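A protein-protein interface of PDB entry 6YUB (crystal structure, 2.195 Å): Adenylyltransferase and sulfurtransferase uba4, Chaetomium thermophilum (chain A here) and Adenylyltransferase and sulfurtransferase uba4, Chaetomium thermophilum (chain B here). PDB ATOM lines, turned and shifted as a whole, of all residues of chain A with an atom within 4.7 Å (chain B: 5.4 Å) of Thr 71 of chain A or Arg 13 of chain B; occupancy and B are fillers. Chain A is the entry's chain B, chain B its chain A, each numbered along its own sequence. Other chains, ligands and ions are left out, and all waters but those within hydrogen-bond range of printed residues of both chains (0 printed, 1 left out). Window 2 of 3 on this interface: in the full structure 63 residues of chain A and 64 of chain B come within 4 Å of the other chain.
NH2 of Arg 13 of chain B lies within hydrogen-bond range of OG1 of Thr 82 of chain A, 2.9 Å away. The guanidinium group (NH2) of Arg 16 of chain B is in salt-bridge range of the side-chain carboxylate (OE1) of Glu 70 of chain A, 3.6 Å away. NE of Arg 16 of chain B lies within hydrogen-bond range of OG of Ser 72 of chain A, at 3.0 Å. The guanidinium group (NH1) of Arg 16 of chain B lies within hydrogen-bond range of the side-chain amide oxygen (OD1) of Asn 73 of chain A (3.2 Å). O of Ile 99 of chain B sits at hydrogen-bond distance from OG1 of Thr 82 of chain A (3.2 Å).
OG of Ser 15 of chain B lies close to O of Ile 11 of chain B (3.3 Å). OG of Ser 15 of chain B is in hydrogen-bond range of O of Glu 12 of chain B, at 2.9 Å. The guanidinium group (NH1) of Arg 13 of chain B sits at hydrogen-bond distance from the backbone carbonyl oxygen (O) of Ile 99 of chain B. The side-chain carboxylate of Glu 70 of chain A sits at hydrogen-bond distance from the side-chain amide nitrogen of Asn 73 of chain A (3.3 Å).
Arg 13 of chain B touches Thr 71 of chain A (NE to CG2, 3.9 Å). Ser 72 of chain A touches Glu 12 of chain B. Ser 72 of chain A touches Arg 13 of chain B. CB of Ser 72 of chain A touches OG of Ser 15 of chain B (3.9 Å). CD1 of Leu 74 of chain A touches NH1 of Arg 13 of chain B, 3.5 Å away. CD1 of Leu 74 of chain A touches O of Ile 99 of chain B (3.5 Å). OG1 of Thr 82 of chain A touches CD of Pro 101 of chain B, at 3.6 Å.
Printed residues of chain B within 4 Å of Glu 70 of chain A: Arg 16 (3.6 Å). Thr 71 of chain A touches just one residue of chain B: Arg 13 (3.9 Å). Of the printed residues of chain A, Glu 12 of chain B touches Ser 72 (3.2 Å). Arg 13 of chain B touches just these residues of chain A: Thr 71, Ser 72, Leu 74 and Thr 82. The nearest residue of chain B that does not touch Thr 71 of chain A is Glu 12 of chain B (4.3 Å). The nearest printed residue of chain A that does not touch Ile 99 of chain B is Thr 71 of chain A (6.4 Å).
Printed residues of chain B that touch a printed residue of chain A: Glu 12, Arg 13, Ser 15, Arg 16, Ile 99 and Pro 101. Hydrophobic or aromatic side chains of chain B within 4 Å of the printed part of chain A: Pro 101. Of the 8 printed residues of chain A, 6 touch a printed residue of chain B. Printed residues of chain A that touch a printed residue of chain B: Glu 70, Thr 71, Ser 72, Asn 73, Leu 74 and Thr 82. Among the printed residues, Asp or Glu carboxylates within 4 Å of a Lys or Arg side-chain nitrogen of the other chain: Glu 70 of chain A with Arg 16 of chain B.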
ATOM      1  N   VAL A  69     -30.507 -22.473 -13.594  1.00  0.00           N
ATOM      2  CA  VAL A  69     -29.776 -22.560 -12.336  1.00  0.00           C
ATOM      3  C   VAL A  69     -29.378 -21.165 -11.875  1.00  0.00           C
ATOM      4  O   VAL A  69     -28.909 -20.334 -12.670  1.00  0.00           O
ATOM      5  CB  VAL A  69     -28.539 -23.461 -12.501  1.00  0.00           C
ATOM      6  CG1 VAL A  69     -27.667 -23.430 -11.248  1.00  0.00           C
ATOM      7  CG2 VAL A  69     -28.967 -24.888 -12.831  1.00  0.00           C
ATOM      8  N   GLU A  70     -29.559 -20.900 -10.584  1.00  0.00           N
ATOM      9  CA  GLU A  70     -29.216 -19.619  -9.985  1.00  0.00           C
ATOM     10  C   GLU A  70     -28.336 -19.843  -8.765  1.00  0.00           C
ATOM     11  O   GLU A  70     -28.439 -20.866  -8.083  1.00  0.00           O
ATOM     12  CB  GLU A  70     -30.470 -18.828  -9.580  1.00  0.00           C
ATOM     13  CG  GLU A  70     -31.322 -18.374 -10.749  1.00  0.00           C
ATOM     14  CD  GLU A  70     -32.582 -17.645 -10.310  1.00  0.00           C
ATOM     15  OE1 GLU A  70     -33.340 -18.199  -9.486  1.00  0.00           O
ATOM     16  OE2 GLU A  70     -32.810 -16.515 -10.786  1.00  0.00           O
ATOM     17  N   THR A  71     -27.470 -18.863  -8.492  1.00  0.00           N
ATOM     18  CA  THR A  71     -26.523 -18.987  -7.391  1.00  0.00           C
ATOM     19  C   THR A  71     -27.236 -19.059  -6.048  1.00  0.00           C
ATOM     20  O   THR A  71     -26.812 -19.798  -5.149  1.00  0.00           O
ATOM     21  CB  THR A  71     -25.550 -17.805  -7.408  1.00  0.00           C
ATOM     22  OG1 THR A  71     -24.922 -17.722  -8.693  1.00  0.00           O
ATOM     23  CG2 THR A  71     -24.485 -17.964  -6.324  1.00  0.00           C
ATOM     24  N   SER A  72     -28.319 -18.299  -5.891  1.00  0.00           N
ATOM     25  CA  SER A  72     -29.009 -18.196  -4.611  1.00  0.00           C
ATOM     26  C   SER A  72     -29.817 -19.436  -4.258  1.00  0.00           C
ATOM     27  O   SER A  72     -30.376 -19.482  -3.158  1.00  0.00           O
ATOM     28  CB  SER A  72     -29.927 -16.970  -4.626  1.00  0.00           C
ATOM     29  OG  SER A  72     -30.845 -17.036  -5.705  1.00  0.00           O
ATOM     30  N   ASN A  73     -29.899 -20.427  -5.143  1.00  0.00           N
ATOM     31  CA  ASN A  73     -30.625 -21.657  -4.862  1.00  0.00           C
ATOM     32  C   ASN A  73     -29.707 -22.852  -4.635  1.00  0.00           C
ATOM     33  O   ASN A  73     -30.199 -23.952  -4.356  1.00  0.00           O
ATOM     34  CB  ASN A  73     -31.595 -21.974  -6.009  1.00  0.00           C
ATOM     35  CG  ASN A  73     -32.701 -20.944  -6.140  1.00  0.00           C
ATOM     36  OD1 ASN A  73     -33.106 -20.321  -5.158  1.00  0.00           O
ATOM     37  ND2 ASN A  73     -33.198 -20.761  -7.358  1.00  0.00           N
ATOM     38  N   LEU A  74     -28.389 -22.668  -4.738  1.00  0.00           N
ATOM     39  CA  LEU A  74     -27.478 -23.800  -4.629  1.00  0.00           C
ATOM     40  C   LEU A  74     -27.480 -24.396  -3.228  1.00  0.00           C
ATOM     41  O   LEU A  74     -27.234 -25.594  -3.070  1.00  0.00           O
ATOM     42  CB  LEU A  74     -26.066 -23.371  -5.029  1.00  0.00           C
ATOM     43  CG  LEU A  74     -25.882 -23.043  -6.511  1.00  0.00           C
ATOM     44  CD1 LEU A  74     -24.504 -22.446  -6.771  1.00  0.00           C
ATOM     45  CD2 LEU A  74     -26.096 -24.285  -7.364  1.00  0.00           C
ATOM     46  N   THR A  82     -21.831 -24.450  -9.446  1.00  0.00           N
ATOM     47  CA  THR A  82     -21.654 -23.013  -9.614  1.00  0.00           C
ATOM     48  C   THR A  82     -21.318 -22.664 -11.060  1.00  0.00           C
ATOM     49  O   THR A  82     -21.768 -21.639 -11.580  1.00  0.00           O
ATOM     50  CB  THR A  82     -20.560 -22.506  -8.672  1.00  0.00           C
ATOM     51  OG1 THR A  82     -20.939 -22.769  -7.317  1.00  0.00           O
ATOM     52  CG2 THR A  82     -20.339 -21.006  -8.853  1.00  0.00           C
ATOM     53  N   VAL A  85     -24.398 -22.257 -13.451  1.00  0.00           N
ATOM     54  CA  VAL A  85     -25.360 -21.177 -13.295  1.00  0.00           C
ATOM     55  C   VAL A  85     -25.679 -20.592 -14.661  1.00  0.00           C
ATOM     56  O   VAL A  85     -24.781 -20.331 -15.473  1.00  0.00           O
ATOM     57  CB  VAL A  85     -24.817 -20.114 -12.332  1.00  0.00           C
ATOM     58  CG1 VAL A  85     -25.666 -18.850 -12.397  1.00  0.00           C
ATOM     59  CG2 VAL A  85     -24.780 -20.657 -10.911  1.00  0.00           C
ATOM     60  N   LYS B   8     -20.905  -8.595  -1.304  1.00  0.00           N
ATOM     61  CA  LYS B   8     -21.995  -8.616  -2.273  1.00  0.00           C
ATOM     62  C   LYS B   8     -22.218 -10.022  -2.819  1.00  0.00           C
ATOM     63  O   LYS B   8     -23.363 -10.435  -3.034  1.00  0.00           O
ATOM     64  CB  LYS B   8     -21.699  -7.640  -3.412  1.00  0.00           C
ATOM     65  N   GLU B   9     -21.137 -10.771  -3.051  1.00  0.00           N
ATOM     66  CA  GLU B   9     -21.273 -12.126  -3.570  1.00  0.00           C
ATOM     67  C   GLU B   9     -21.958 -13.037  -2.558  1.00  0.00           C
ATOM     68  O   GLU B   9     -22.810 -13.854  -2.927  1.00  0.00           O
ATOM     69  CB  GLU B   9     -19.899 -12.683  -3.945  1.00  0.00           C
ATOM     70  N   GLU B  10     -21.600 -12.912  -1.278  1.00  0.00           N
ATOM     71  CA  GLU B  10     -22.197 -13.764  -0.257  1.00  0.00           C
ATOM     72  C   GLU B  10     -23.660 -13.417  -0.020  1.00  0.00           C
ATOM     73  O   GLU B  10     -24.470 -14.310   0.253  1.00  0.00           O
ATOM     74  CB  GLU B  10     -21.397 -13.649   1.040  1.00  0.00           C
ATOM     75  CG  GLU B  10     -19.942 -14.068   0.896  1.00  0.00           C
ATOM     76  CD  GLU B  10     -19.117 -13.766   2.130  1.00  0.00           C
ATOM     77  OE1 GLU B  10     -19.278 -12.669   2.705  1.00  0.00           O
ATOM     78  OE2 GLU B  10     -18.310 -14.631   2.530  1.00  0.00           O
ATOM     79  N   ILE B  11     -24.021 -12.137  -0.125  1.00  0.00           N
ATOM     80  CA  ILE B  11     -25.420 -11.747   0.019  1.00  0.00           C
ATOM     81  C   ILE B  11     -26.262 -12.379  -1.081  1.00  0.00           C
ATOM     82  O   ILE B  11     -27.391 -12.822  -0.842  1.00  0.00           O
ATOM     83  CB  ILE B  11     -25.550 -10.212   0.022  1.00  0.00           C
ATOM     84  CG1 ILE B  11     -24.918  -9.635   1.292  1.00  0.00           C
ATOM     85  CG2 ILE B  11     -27.011  -9.803  -0.089  1.00  0.00           C
ATOM     86  CD1 ILE B  11     -24.707  -8.132   1.247  1.00  0.00           C
ATOM     87  N   GLU B  12     -25.728 -12.438  -2.301  1.00  0.00           N
ATOM     88  CA  GLU B  12     -26.451 -13.078  -3.394  1.00  0.00           C
ATOM     89  C   GLU B  12     -26.631 -14.568  -3.134  1.00  0.00           C
ATOM     90  O   GLU B  12     -27.741 -15.101  -3.242  1.00  0.00           O
ATOM     91  CB  GLU B  12     -25.711 -12.856  -4.714  1.00  0.00           C
ATOM     92  CG  GLU B  12     -26.129 -13.816  -5.818  1.00  0.00           C
ATOM     93  CD  GLU B  12     -25.596 -13.413  -7.180  1.00  0.00           C
ATOM     94  OE1 GLU B  12     -24.360 -13.417  -7.366  1.00  0.00           O
ATOM     95  OE2 GLU B  12     -26.419 -13.079  -8.060  1.00  0.00           O
ATOM     96  N   ARG B  13     -25.542 -15.259  -2.790  1.00  0.00           N
ATOM     97  CA  ARG B  13     -25.595 -16.711  -2.652  1.00  0.00           C
ATOM     98  C   ARG B  13     -26.507 -17.136  -1.507  1.00  0.00           C
ATOM     99  O   ARG B  13     -27.194 -18.159  -1.601  1.00  0.00           O
ATOM    100  CB  ARG B  13     -24.184 -17.262  -2.445  1.00  0.00           C
ATOM    101  CG  ARG B  13     -24.123 -18.763  -2.222  1.00  0.00           C
ATOM    102  CD  ARG B  13     -22.688 -19.277  -2.209  1.00  0.00           C
ATOM    103  NE  ARG B  13     -22.134 -19.421  -3.550  1.00  0.00           N
ATOM    104  CZ  ARG B  13     -22.195 -20.537  -4.274  1.00  0.00           C
ATOM    105  NH1 ARG B  13     -22.790 -21.618  -3.792  1.00  0.00           N
ATOM    106  NH2 ARG B  13     -21.656 -20.570  -5.486  1.00  0.00           N
ATOM    107  N   TYR B  14     -26.529 -16.364  -0.420  1.00  0.00           N
ATOM    108  CA  TYR B  14     -27.204 -16.771   0.806  1.00  0.00           C
ATOM    109  C   TYR B  14     -28.486 -15.993   1.078  1.00  0.00           C
ATOM    110  O   TYR B  14     -29.098 -16.187   2.134  1.00  0.00           O
ATOM    111  CB  TYR B  14     -26.247 -16.622   1.994  1.00  0.00           C
ATOM    112  CG  TYR B  14     -24.977 -17.434   1.857  1.00  0.00           C
ATOM    113  CD1 TYR B  14     -25.030 -18.783   1.536  1.00  0.00           C
ATOM    114  CD2 TYR B  14     -23.732 -16.854   2.037  1.00  0.00           C
ATOM    115  CE1 TYR B  14     -23.884 -19.533   1.401  1.00  0.00           C
ATOM    116  CE2 TYR B  14     -22.571 -17.597   1.905  1.00  0.00           C
ATOM    117  CZ  TYR B  14     -22.656 -18.938   1.586  1.00  0.00           C
ATOM    118  OH  TYR B  14     -21.512 -19.690   1.447  1.00  0.00           O
ATOM    119  N   SER B  15     -28.915 -15.132   0.153  1.00  0.00           N
ATOM    120  CA  SER B  15     -30.072 -14.278   0.410  1.00  0.00           C
ATOM    121  C   SER B  15     -31.307 -15.097   0.767  1.00  0.00           C
ATOM    122  O   SER B  15     -31.973 -14.829   1.774  1.00  0.00           O
ATOM    123  CB  SER B  15     -30.348 -13.397  -0.811  1.00  0.00           C
ATOM    124  OG  SER B  15     -30.168 -14.124  -2.017  1.00  0.00           O
ATOM    125  N   ARG B  16     -31.637 -16.098  -0.049  1.00  0.00           N
ATOM    126  CA  ARG B  16     -32.868 -16.857   0.145  1.00  0.00           C
ATOM    127  C   ARG B  16     -32.803 -17.794   1.340  1.00  0.00           C
ATOM    128  O   ARG B  16     -33.841 -18.338   1.734  1.00  0.00           O
ATOM    129  CB  ARG B  16     -33.188 -17.638  -1.130  1.00  0.00           C
ATOM    130  CG  ARG B  16     -33.223 -16.745  -2.360  1.00  0.00           C
ATOM    131  CD  ARG B  16     -33.639 -17.482  -3.615  1.00  0.00           C
ATOM    132  NE  ARG B  16     -33.621 -16.584  -4.768  1.00  0.00           N
ATOM    133  CZ  ARG B  16     -34.282 -16.796  -5.900  1.00  0.00           C
ATOM    134  NH1 ARG B  16     -35.032 -17.881  -6.044  1.00  0.00           N
ATOM    135  NH2 ARG B  16     -34.200 -15.915  -6.888  1.00  0.00           N
ATOM    136  N   GLY B  54     -23.500 -26.267   0.895  1.00  0.00           N
ATOM    137  CA  GLY B  54     -24.427 -25.310   0.316  1.00  0.00           C
ATOM    138  C   GLY B  54     -24.823 -24.222   1.290  1.00  0.00           C
ATOM    139  O   GLY B  54     -24.903 -23.047   0.924  1.00  0.00           O
ATOM    140  N   ILE B  99     -20.724 -27.215  -5.729  1.00  0.00           N
ATOM    141  CA  ILE B  99     -21.882 -26.626  -5.060  1.00  0.00           C
ATOM    142  C   ILE B  99     -21.549 -25.223  -4.557  1.00  0.00           C
ATOM    143  O   ILE B  99     -22.298 -24.263  -4.788  1.00  0.00           O
ATOM    144  CB  ILE B  99     -22.355 -27.528  -3.908  1.00  0.00           C
ATOM    145  CG1 ILE B  99     -22.897 -28.855  -4.445  1.00  0.00           C
ATOM    146  CG2 ILE B  99     -23.417 -26.807  -3.079  1.00  0.00           C
ATOM    147  CD1 ILE B  99     -23.127 -29.884  -3.373  1.00  0.00           C
ATOM    148  N   ASN B 100     -20.419 -25.082  -3.866  1.00  0.00           N
ATOM    149  CA  ASN B 100     -20.070 -23.822  -3.217  1.00  0.00           C
ATOM    150  C   ASN B 100     -18.559 -23.736  -3.034  1.00  0.00           C
ATOM    151  O   ASN B 100     -17.990 -24.479  -2.224  1.00  0.00           O
ATOM    152  CB  ASN B 100     -20.781 -23.716  -1.867  1.00  0.00           C
ATOM    153  CG  ASN B 100     -20.645 -22.345  -1.241  1.00  0.00           C
ATOM    154  OD1 ASN B 100     -19.880 -21.505  -1.710  1.00  0.00           O
ATOM    155  ND2 ASN B 100     -21.393 -22.113  -0.158  1.00  0.00           N
ATOM    156  N   PRO B 101     -17.872 -22.855  -3.769  1.00  0.00           N
ATOM    157  CA  PRO B 101     -16.413 -22.758  -3.633  1.00  0.00           C
ATOM    158  C   PRO B 101     -15.944 -21.875  -2.488  1.00  0.00           C
ATOM    159  O   PRO B 101     -14.732 -21.757  -2.282  1.00  0.00           O
ATOM    160  CB  PRO B 101     -15.987 -22.163  -4.989  1.00  0.00           C
ATOM    161  CG  PRO B 101     -17.140 -21.293  -5.376  1.00  0.00           C
ATOM    162  CD  PRO B 101     -18.389 -21.989  -4.852  1.00  0.00           C
ATOM    163  N   LEU B 102     -16.851 -21.269  -1.730  1.00  0.00           N
ATOM    164  CA  LEU B 102     -16.454 -20.292  -0.725  1.00  0.00           C
ATOM    165  C   LEU B 102     -15.915 -20.930   0.550  1.00  0.00           C
ATOM    166  O   LEU B 102     -14.998 -20.373   1.167  1.00  0.00           O
ATOM    167  CB  LEU B 102     -17.639 -19.378  -0.392  1.00  0.00           C
ATOM    168  CG  LEU B 102     -18.218 -18.589  -1.571  1.00  0.00           C
ATOM    169  CD1 LEU B 102     -19.273 -17.596  -1.093  1.00  0.00           C
ATOM    170  CD2 LEU B 102     -17.119 -17.873  -2.344  1.00  0.00           C
